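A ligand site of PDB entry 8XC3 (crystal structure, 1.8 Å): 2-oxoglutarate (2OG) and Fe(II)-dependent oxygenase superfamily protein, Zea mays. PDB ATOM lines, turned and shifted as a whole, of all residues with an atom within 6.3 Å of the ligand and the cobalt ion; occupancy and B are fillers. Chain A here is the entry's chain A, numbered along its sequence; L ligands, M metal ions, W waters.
Merely in contact with the ligand: Phe 301, Val 287, Leu 237, Leu 246 and Ile 225. Hydrophobic or aromatic side chains within 4 Å of the ligand: Tyr 213, Ile 225, His 228, Leu 237, Leu 246, His 285, Val 287 and Phe 301. 13 residues have an atom within 4 Å of the ligand: Arg 209, Asn 211, Tyr 213, Ile 225, His 228, Asp 230, Leu 237, Leu 246, His 285, Val 287, Arg 295, Ser 297 and Phe 301.
A ring nitrogen (NE2) of His 228 binds the cobalt ion. The cobalt ion is bound by NE2 of His 285, 2.1 Å away. O3 of the ligand is bound to the cobalt ion (2.2 Å). OD1 of Asp 230 binds the cobalt ion. An oxygen (O2) of the ligand is bound to the cobalt ion. The cobalt ion is bound by water W1 (2.3 Å).
The side-chain carboxylate of Asp 230 sits at hydrogen-bond distance from the side-chain amide nitrogen of Asn 267, 3.1 Å away. OG1 of Thr 235 sits at hydrogen-bond distance from OD2 of Asp 230 (2.7 Å). N of Asn 211 sits at hydrogen-bond distance from O of Ser 297 (2.8 Å). The backbone carbonyl oxygen of Arg 295 is in hydrogen-bond range of the backbone NH of Tyr 213 (2.8 Å). OD1 of Asn 211 is in hydrogen-bond range of NE of Arg 209, at 2.7 Å. OD1 of Asn 211 lies within hydrogen-bond range of NE2 of Gln 138, at 2.7 Å. The backbone carbonyl oxygen of Arg 209 is in hydrogen-bond range of the backbone NH of Ala 299 (2.8 Å). OE1 of Gln 138 sits at hydrogen-bond distance from NH2 of Arg 209.
The side-chain hydroxyl (OG) of Ser 297 is in hydrogen-bond range of an oxygen (O4) of the ligand. O5 of the ligand lies within salt-bridge range of NH2 of Arg 295 (2.7 Å). The side-chain hydroxyl (OH) of Tyr 213 lies within hydrogen-bond range of an oxygen (O4) of the ligand. O1 of the ligand sits at hydrogen-bond distance from ND2 of Asn 211 (3.2 Å). The guanidinium group (NE) of Arg 209 lies within salt-bridge range of an oxygen (O1) of the ligand.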
ATOM      1  N   GLN A 138     -24.645  20.561  -6.034  1.00  0.00           N
ATOM      2  CA  GLN A 138     -23.857  21.114  -4.934  1.00  0.00           C
ATOM      3  C   GLN A 138     -24.731  21.343  -3.725  1.00  0.00           C
ATOM      4  O   GLN A 138     -25.956  21.504  -3.821  1.00  0.00           O
ATOM      5  CB  GLN A 138     -23.167  22.434  -5.311  1.00  0.00           C
ATOM      6  CG  GLN A 138     -24.143  23.586  -5.552  1.00  0.00           C
ATOM      7  CD  GLN A 138     -23.926  24.741  -4.598  1.00  0.00           C
ATOM      8  OE1 GLN A 138     -24.867  25.195  -3.947  1.00  0.00           O
ATOM      9  NE2 GLN A 138     -22.694  25.216  -4.512  1.00  0.00           N
ATOM     10  N   ARG A 209     -19.808  31.897   1.586  1.00  0.00           N
ATOM     11  CA  ARG A 209     -20.493  30.781   0.952  1.00  0.00           C
ATOM     12  C   ARG A 209     -19.490  29.654   0.778  1.00  0.00           C
ATOM     13  O   ARG A 209     -18.548  29.764  -0.024  1.00  0.00           O
ATOM     14  CB  ARG A 209     -21.124  31.193  -0.389  1.00  0.00           C
ATOM     15  CG  ARG A 209     -21.894  30.040  -1.059  1.00  0.00           C
ATOM     16  CD  ARG A 209     -22.503  30.483  -2.398  1.00  0.00           C
ATOM     17  NE  ARG A 209     -23.078  29.353  -3.123  1.00  0.00           N
ATOM     18  CZ  ARG A 209     -24.374  29.186  -3.373  1.00  0.00           C
ATOM     19  NH1 ARG A 209     -25.255  30.086  -2.973  1.00  0.00           N
ATOM     20  NH2 ARG A 209     -24.790  28.106  -4.042  1.00  0.00           N
ATOM     21  N   ASN A 211     -19.026  26.233  -0.693  1.00  0.00           N
ATOM     22  CA  ASN A 211     -19.654  25.347  -1.665  1.00  0.00           C
ATOM     23  C   ASN A 211     -19.076  23.939  -1.555  1.00  0.00           C
ATOM     24  O   ASN A 211     -17.863  23.755  -1.474  1.00  0.00           O
ATOM     25  CB  ASN A 211     -19.477  25.841  -3.087  1.00  0.00           C
ATOM     26  CG  ASN A 211     -20.149  27.168  -3.317  1.00  0.00           C
ATOM     27  OD1 ASN A 211     -21.370  27.271  -3.272  1.00  0.00           O
ATOM     28  ND2 ASN A 211     -19.347  28.197  -3.558  1.00  0.00           N
ATOM     29  N   TYR A 213     -19.209  20.512  -3.815  1.00  0.00           N
ATOM     30  CA  TYR A 213     -19.611  19.848  -5.051  1.00  0.00           C
ATOM     31  C   TYR A 213     -19.278  18.355  -4.962  1.00  0.00           C
ATOM     32  O   TYR A 213     -18.108  17.988  -5.071  1.00  0.00           O
ATOM     33  CB  TYR A 213     -18.908  20.459  -6.263  1.00  0.00           C
ATOM     34  CG  TYR A 213     -19.068  21.964  -6.343  1.00  0.00           C
ATOM     35  CD1 TYR A 213     -18.168  22.814  -5.731  1.00  0.00           C
ATOM     36  CD2 TYR A 213     -20.115  22.532  -7.074  1.00  0.00           C
ATOM     37  CE1 TYR A 213     -18.320  24.208  -5.814  1.00  0.00           C
ATOM     38  CE2 TYR A 213     -20.287  23.916  -7.153  1.00  0.00           C
ATOM     39  CZ  TYR A 213     -19.386  24.747  -6.538  1.00  0.00           C
ATOM     40  OH  TYR A 213     -19.559  26.119  -6.626  1.00  0.00           O
ATOM     41  N   ILE A 225     -22.383  24.544 -10.284  1.00  0.00           N
ATOM     42  CA  ILE A 225     -23.179  25.740 -10.063  1.00  0.00           C
ATOM     43  C   ILE A 225     -23.407  26.362 -11.430  1.00  0.00           C
ATOM     44  O   ILE A 225     -22.477  26.449 -12.248  1.00  0.00           O
ATOM     45  CB  ILE A 225     -22.505  26.704  -9.047  1.00  0.00           C
ATOM     46  CG1 ILE A 225     -23.529  27.681  -8.480  1.00  0.00           C
ATOM     47  CG2 ILE A 225     -21.320  27.419  -9.615  1.00  0.00           C
ATOM     48  CD1 ILE A 225     -22.972  28.555  -7.325  1.00  0.00           C
ATOM     49  N   HIS A 228     -23.794  32.147 -13.949  1.00  0.00           N
ATOM     50  CA  HIS A 228     -24.305  33.303 -13.222  1.00  0.00           C
ATOM     51  C   HIS A 228     -23.207  34.344 -13.140  1.00  0.00           C
ATOM     52  O   HIS A 228     -22.024  34.046 -13.323  1.00  0.00           O
ATOM     53  CB  HIS A 228     -24.763  32.928 -11.809  1.00  0.00           C
ATOM     54  CG  HIS A 228     -23.624  32.591 -10.901  1.00  0.00           C
ATOM     55  ND1 HIS A 228     -23.015  31.350 -10.892  1.00  0.00           N
ATOM     56  CD2 HIS A 228     -22.991  33.321  -9.956  1.00  0.00           C
ATOM     57  CE1 HIS A 228     -22.055  31.334  -9.996  1.00  0.00           C
ATOM     58  NE2 HIS A 228     -22.009  32.530  -9.417  1.00  0.00           N
ATOM     59  N   SER A 229     -23.613  35.574 -12.844  1.00  0.00           N
ATOM     60  CA  SER A 229     -22.723  36.598 -12.350  1.00  0.00           C
ATOM     61  C   SER A 229     -23.077  36.867 -10.898  1.00  0.00           C
ATOM     62  O   SER A 229     -24.242  36.745 -10.487  1.00  0.00           O
ATOM     63  CB  SER A 229     -22.796  37.892 -13.190  1.00  0.00           C
ATOM     64  OG  SER A 229     -24.129  38.366 -13.294  1.00  0.00           O
ATOM     65  N   ASP A 230     -22.063  37.180 -10.101  1.00  0.00           N
ATOM     66  CA  ASP A 230     -22.304  37.551  -8.718  1.00  0.00           C
ATOM     67  C   ASP A 230     -22.942  38.946  -8.647  1.00  0.00           C
ATOM     68  O   ASP A 230     -22.635  39.832  -9.453  1.00  0.00           O
ATOM     69  CB  ASP A 230     -20.992  37.521  -7.919  1.00  0.00           C
ATOM     70  CG  ASP A 230     -20.359  36.146  -7.860  1.00  0.00           C
ATOM     71  OD1 ASP A 230     -21.011  35.148  -8.201  1.00  0.00           O
ATOM     72  OD2 ASP A 230     -19.166  36.065  -7.508  1.00  0.00           O
ATOM     73  N   THR A 235     -16.073  39.734  -5.343  1.00  0.00           N
ATOM     74  CA  THR A 235     -16.016  38.400  -4.749  1.00  0.00           C
ATOM     75  C   THR A 235     -14.559  37.992  -4.619  1.00  0.00           C
ATOM     76  O   THR A 235     -13.761  38.152  -5.545  1.00  0.00           O
ATOM     77  CB  THR A 235     -16.744  37.390  -5.609  1.00  0.00           C
ATOM     78  OG1 THR A 235     -18.144  37.720  -5.663  1.00  0.00           O
ATOM     79  CG2 THR A 235     -16.600  35.944  -5.028  1.00  0.00           C
ATOM     80  N   LEU A 237     -12.496  34.558  -3.919  1.00  0.00           N
ATOM     81  CA  LEU A 237     -12.794  33.127  -3.995  1.00  0.00           C
ATOM     82  C   LEU A 237     -11.554  32.311  -3.684  1.00  0.00           C
ATOM     83  O   LEU A 237     -10.470  32.578  -4.201  1.00  0.00           O
ATOM     84  CB  LEU A 237     -13.329  32.772  -5.388  1.00  0.00           C
ATOM     85  CG  LEU A 237     -13.592  31.269  -5.598  1.00  0.00           C
ATOM     86  CD1 LEU A 237     -14.903  30.845  -4.920  1.00  0.00           C
ATOM     87  CD2 LEU A 237     -13.595  30.939  -7.104  1.00  0.00           C
ATOM     88  N   LEU A 238     -11.741  31.277  -2.857  1.00  0.00           N
ATOM     89  CA  LEU A 238     -10.679  30.335  -2.507  1.00  0.00           C
ATOM     90  C   LEU A 238     -11.151  28.935  -2.895  1.00  0.00           C
ATOM     91  O   LEU A 238     -12.240  28.517  -2.496  1.00  0.00           O
ATOM     92  CB  LEU A 238     -10.367  30.423  -1.007  1.00  0.00           C
ATOM     93  CG  LEU A 238      -9.465  29.323  -0.431  1.00  0.00           C
ATOM     94  CD1 LEU A 238      -8.122  29.348  -1.141  1.00  0.00           C
ATOM     95  CD2 LEU A 238      -9.312  29.523   1.079  1.00  0.00           C
ATOM     96  N   VAL A 239     -10.363  28.249  -3.727  1.00  0.00           N
ATOM     97  CA  VAL A 239     -10.688  26.892  -4.168  1.00  0.00           C
ATOM     98  C   VAL A 239      -9.742  25.923  -3.475  1.00  0.00           C
ATOM     99  O   VAL A 239      -8.523  26.020  -3.663  1.00  0.00           O
ATOM    100  CB  VAL A 239     -10.551  26.741  -5.696  1.00  0.00           C
ATOM    101  CG1 VAL A 239     -10.783  25.241  -6.084  1.00  0.00           C
ATOM    102  CG2 VAL A 239     -11.490  27.668  -6.404  1.00  0.00           C
ATOM    103  N   GLY A 245     -12.773  23.046 -12.138  1.00  0.00           N
ATOM    104  CA  GLY A 245     -14.216  23.121 -12.197  1.00  0.00           C
ATOM    105  C   GLY A 245     -14.687  24.500 -12.620  1.00  0.00           C
ATOM    106  O   GLY A 245     -15.642  24.636 -13.394  1.00  0.00           O
ATOM    107  N   LEU A 246     -14.017  25.533 -12.124  1.00  0.00           N
ATOM    108  CA  LEU A 246     -14.443  26.904 -12.408  1.00  0.00           C
ATOM    109  C   LEU A 246     -14.150  27.283 -13.855  1.00  0.00           C
ATOM    110  O   LEU A 246     -13.028  27.087 -14.353  1.00  0.00           O
ATOM    111  CB  LEU A 246     -13.766  27.868 -11.454  1.00  0.00           C
ATOM    112  CG  LEU A 246     -14.194  29.329 -11.681  1.00  0.00           C
ATOM    113  CD1 LEU A 246     -15.694  29.474 -11.429  1.00  0.00           C
ATOM    114  CD2 LEU A 246     -13.430  30.229 -10.756  1.00  0.00           C
ATOM    115  N   ASN A 267     -13.198  38.415  -8.500  1.00  0.00           N
ATOM    116  CA  ASN A 267     -14.050  38.705  -9.645  1.00  0.00           C
ATOM    117  C   ASN A 267     -15.024  39.820  -9.289  1.00  0.00           C
ATOM    118  O   ASN A 267     -15.442  39.951  -8.134  1.00  0.00           O
ATOM    119  CB  ASN A 267     -14.814  37.456 -10.158  1.00  0.00           C
ATOM    120  CG  ASN A 267     -15.865  36.945  -9.198  1.00  0.00           C
ATOM    121  OD1 ASN A 267     -15.583  36.101  -8.341  1.00  0.00           O
ATOM    122  ND2 ASN A 267     -17.107  37.396  -9.390  1.00  0.00           N
ATOM    123  N   HIS A 285     -19.871  33.140 -14.818  1.00  0.00           N
ATOM    124  CA  HIS A 285     -19.026  32.000 -14.494  1.00  0.00           C
ATOM    125  C   HIS A 285     -19.881  30.809 -14.069  1.00  0.00           C
ATOM    126  O   HIS A 285     -21.085  30.941 -13.776  1.00  0.00           O
ATOM    127  CB  HIS A 285     -18.001  32.369 -13.411  1.00  0.00           C
ATOM    128  CG  HIS A 285     -18.587  32.997 -12.185  1.00  0.00           C
ATOM    129  ND1 HIS A 285     -18.926  34.331 -12.126  1.00  0.00           N
ATOM    130  CD2 HIS A 285     -18.887  32.478 -10.980  1.00  0.00           C
ATOM    131  CE1 HIS A 285     -19.397  34.612 -10.918  1.00  0.00           C
ATOM    132  NE2 HIS A 285     -19.396  33.489 -10.210  1.00  0.00           N
ATOM    133  N   ARG A 286     -19.249  29.641 -14.043  1.00  0.00           N
ATOM    134  CA  ARG A 286     -19.935  28.382 -13.728  1.00  0.00           C
ATOM    135  C   ARG A 286     -18.935  27.388 -13.189  1.00  0.00           C
ATOM    136  O   ARG A 286     -17.724  27.530 -13.353  1.00  0.00           O
ATOM    137  CB  ARG A 286     -20.657  27.790 -14.950  1.00  0.00           C
ATOM    138  CG  ARG A 286     -19.722  27.249 -16.025  1.00  0.00           C
ATOM    139  CD  ARG A 286     -20.518  26.713 -17.207  1.00  0.00           C
ATOM    140  NE  ARG A 286     -19.634  26.057 -18.177  1.00  0.00           N
ATOM    141  CZ  ARG A 286     -20.021  25.669 -19.397  1.00  0.00           C
ATOM    142  NH1 ARG A 286     -21.260  25.860 -19.822  1.00  0.00           N
ATOM    143  NH2 ARG A 286     -19.138  25.099 -20.206  1.00  0.00           N
ATOM    144  N   VAL A 287     -19.465  26.331 -12.566  1.00  0.00           N
ATOM    145  CA  VAL A 287     -18.634  25.235 -12.095  1.00  0.00           C
ATOM    146  C   VAL A 287     -19.160  23.949 -12.719  1.00  0.00           C
ATOM    147  O   VAL A 287     -20.349  23.636 -12.611  1.00  0.00           O
ATOM    148  CB  VAL A 287     -18.612  25.155 -10.557  1.00  0.00           C
ATOM    149  CG1 VAL A 287     -17.937  23.852 -10.107  1.00  0.00           C
ATOM    150  CG2 VAL A 287     -17.842  26.343  -9.984  1.00  0.00           C
ATOM    151  N   ARG A 295     -15.380  18.688  -4.756  1.00  0.00           N
ATOM    152  CA  ARG A 295     -14.727  19.973  -4.909  1.00  0.00           C
ATOM    153  C   ARG A 295     -15.276  20.918  -3.849  1.00  0.00           C
ATOM    154  O   ARG A 295     -16.498  20.940  -3.618  1.00  0.00           O
ATOM    155  CB  ARG A 295     -14.959  20.559  -6.311  1.00  0.00           C
ATOM    156  CG  ARG A 295     -14.272  21.903  -6.538  1.00  0.00           C
ATOM    157  CD  ARG A 295     -14.461  22.341  -7.983  1.00  0.00           C
ATOM    158  NE  ARG A 295     -13.806  23.633  -8.219  1.00  0.00           N
ATOM    159  CZ  ARG A 295     -14.355  24.809  -7.939  1.00  0.00           C
ATOM    160  NH1 ARG A 295     -15.574  24.869  -7.399  1.00  0.00           N
ATOM    161  NH2 ARG A 295     -13.694  25.917  -8.187  1.00  0.00           N
ATOM    162  N   LEU A 296     -14.392  21.663  -3.198  1.00  0.00           N
ATOM    163  CA  LEU A 296     -14.773  22.625  -2.169  1.00  0.00           C
ATOM    164  C   LEU A 296     -14.249  24.021  -2.509  1.00  0.00           C
ATOM    165  O   LEU A 296     -13.068  24.192  -2.868  1.00  0.00           O
ATOM    166  CB  LEU A 296     -14.248  22.230  -0.778  1.00  0.00           C
ATOM    167  CG  LEU A 296     -14.951  21.074  -0.070  1.00  0.00           C
ATOM    168  CD1 LEU A 296     -14.461  19.758  -0.596  1.00  0.00           C
ATOM    169  CD2 LEU A 296     -14.719  21.163   1.439  1.00  0.00           C
ATOM    170  N   SER A 297     -15.106  25.013  -2.360  1.00  0.00           N
ATOM    171  CA  SER A 297     -14.690  26.411  -2.496  1.00  0.00           C
ATOM    172  C   SER A 297     -15.317  27.260  -1.402  1.00  0.00           C
ATOM    173  O   SER A 297     -16.358  26.920  -0.838  1.00  0.00           O
ATOM    174  CB  SER A 297     -15.032  26.999  -3.886  1.00  0.00           C
ATOM    175  OG  SER A 297     -16.437  27.107  -4.057  1.00  0.00           O
ATOM    176  N   LEU A 298     -14.705  28.423  -1.175  1.00  0.00           N
ATOM    177  CA  LEU A 298     -15.248  29.417  -0.256  1.00  0.00           C
ATOM    178  C   LEU A 298     -15.258  30.760  -0.978  1.00  0.00           C
ATOM    179  O   LEU A 298     -14.210  31.256  -1.394  1.00  0.00           O
ATOM    180  CB  LEU A 298     -14.426  29.504   1.036  1.00  0.00           C
ATOM    181  CG  LEU A 298     -14.728  30.727   1.923  1.00  0.00           C
ATOM    182  CD1 LEU A 298     -16.214  30.794   2.319  1.00  0.00           C
ATOM    183  CD2 LEU A 298     -13.873  30.684   3.161  1.00  0.00           C
ATOM    184  N   ALA A 299     -16.450  31.289  -1.187  1.00  0.00           N
ATOM    185  CA  ALA A 299     -16.611  32.607  -1.807  1.00  0.00           C
ATOM    186  C   ALA A 299     -16.955  33.619  -0.719  1.00  0.00           C
ATOM    187  O   ALA A 299     -17.825  33.372   0.107  1.00  0.00           O
ATOM    188  CB  ALA A 299     -17.700  32.575  -2.875  1.00  0.00           C
ATOM    189  N   PHE A 301     -18.508  37.153  -0.614  1.00  0.00           N
ATOM    190  CA  PHE A 301     -19.244  38.128  -1.402  1.00  0.00           C
ATOM    191  C   PHE A 301     -19.268  39.442  -0.652  1.00  0.00           C
ATOM    192  O   PHE A 301     -19.802  39.505   0.466  1.00  0.00           O
ATOM    193  CB  PHE A 301     -20.683  37.688  -1.645  1.00  0.00           C
ATOM    194  CG  PHE A 301     -20.802  36.356  -2.316  1.00  0.00           C
ATOM    195  CD1 PHE A 301     -20.242  36.142  -3.554  1.00  0.00           C
ATOM    196  CD2 PHE A 301     -21.461  35.310  -1.680  1.00  0.00           C
ATOM    197  CE1 PHE A 301     -20.344  34.899  -4.170  1.00  0.00           C
ATOM    198  CE2 PHE A 301     -21.582  34.078  -2.296  1.00  0.00           C
ATOM    199  CZ  PHE A 301     -21.003  33.873  -3.538  1.00  0.00           C
HETATM  200  C1  LIG L   1     -20.431  31.290  -6.173  1.00  0.00           C
HETATM  201  O1  LIG L   1     -20.602  30.706  -5.063  1.00  0.00           O
HETATM  202  O2  LIG L   1     -21.081  32.318  -6.439  1.00  0.00           O
HETATM  203  C2  LIG L   1     -19.440  30.718  -7.187  1.00  0.00           C
HETATM  204  O3  LIG L   1     -19.456  31.085  -8.324  1.00  0.00           O
HETATM  205  C3  LIG L   1     -18.448  29.643  -6.717  1.00  0.00           C
HETATM  206  C4  LIG L   1     -17.496  29.187  -7.827  1.00  0.00           C
HETATM  207  C5  LIG L   1     -16.549  28.065  -7.395  1.00  0.00           C
HETATM  208  O4  LIG L   1     -16.969  27.166  -6.605  1.00  0.00           O
HETATM  209  O5  LIG L   1     -15.348  28.052  -7.828  1.00  0.00           O
HETATM  210 CO    CO M   1     -20.303  33.086  -8.387  1.00  0.00          CO
HETATM  211  O   HOH W   1     -18.375  33.713  -7.362  1.00  0.00           O
HETATM  212  O   HOH W   2     -23.508  32.246  -5.614  1.00  0.00           O
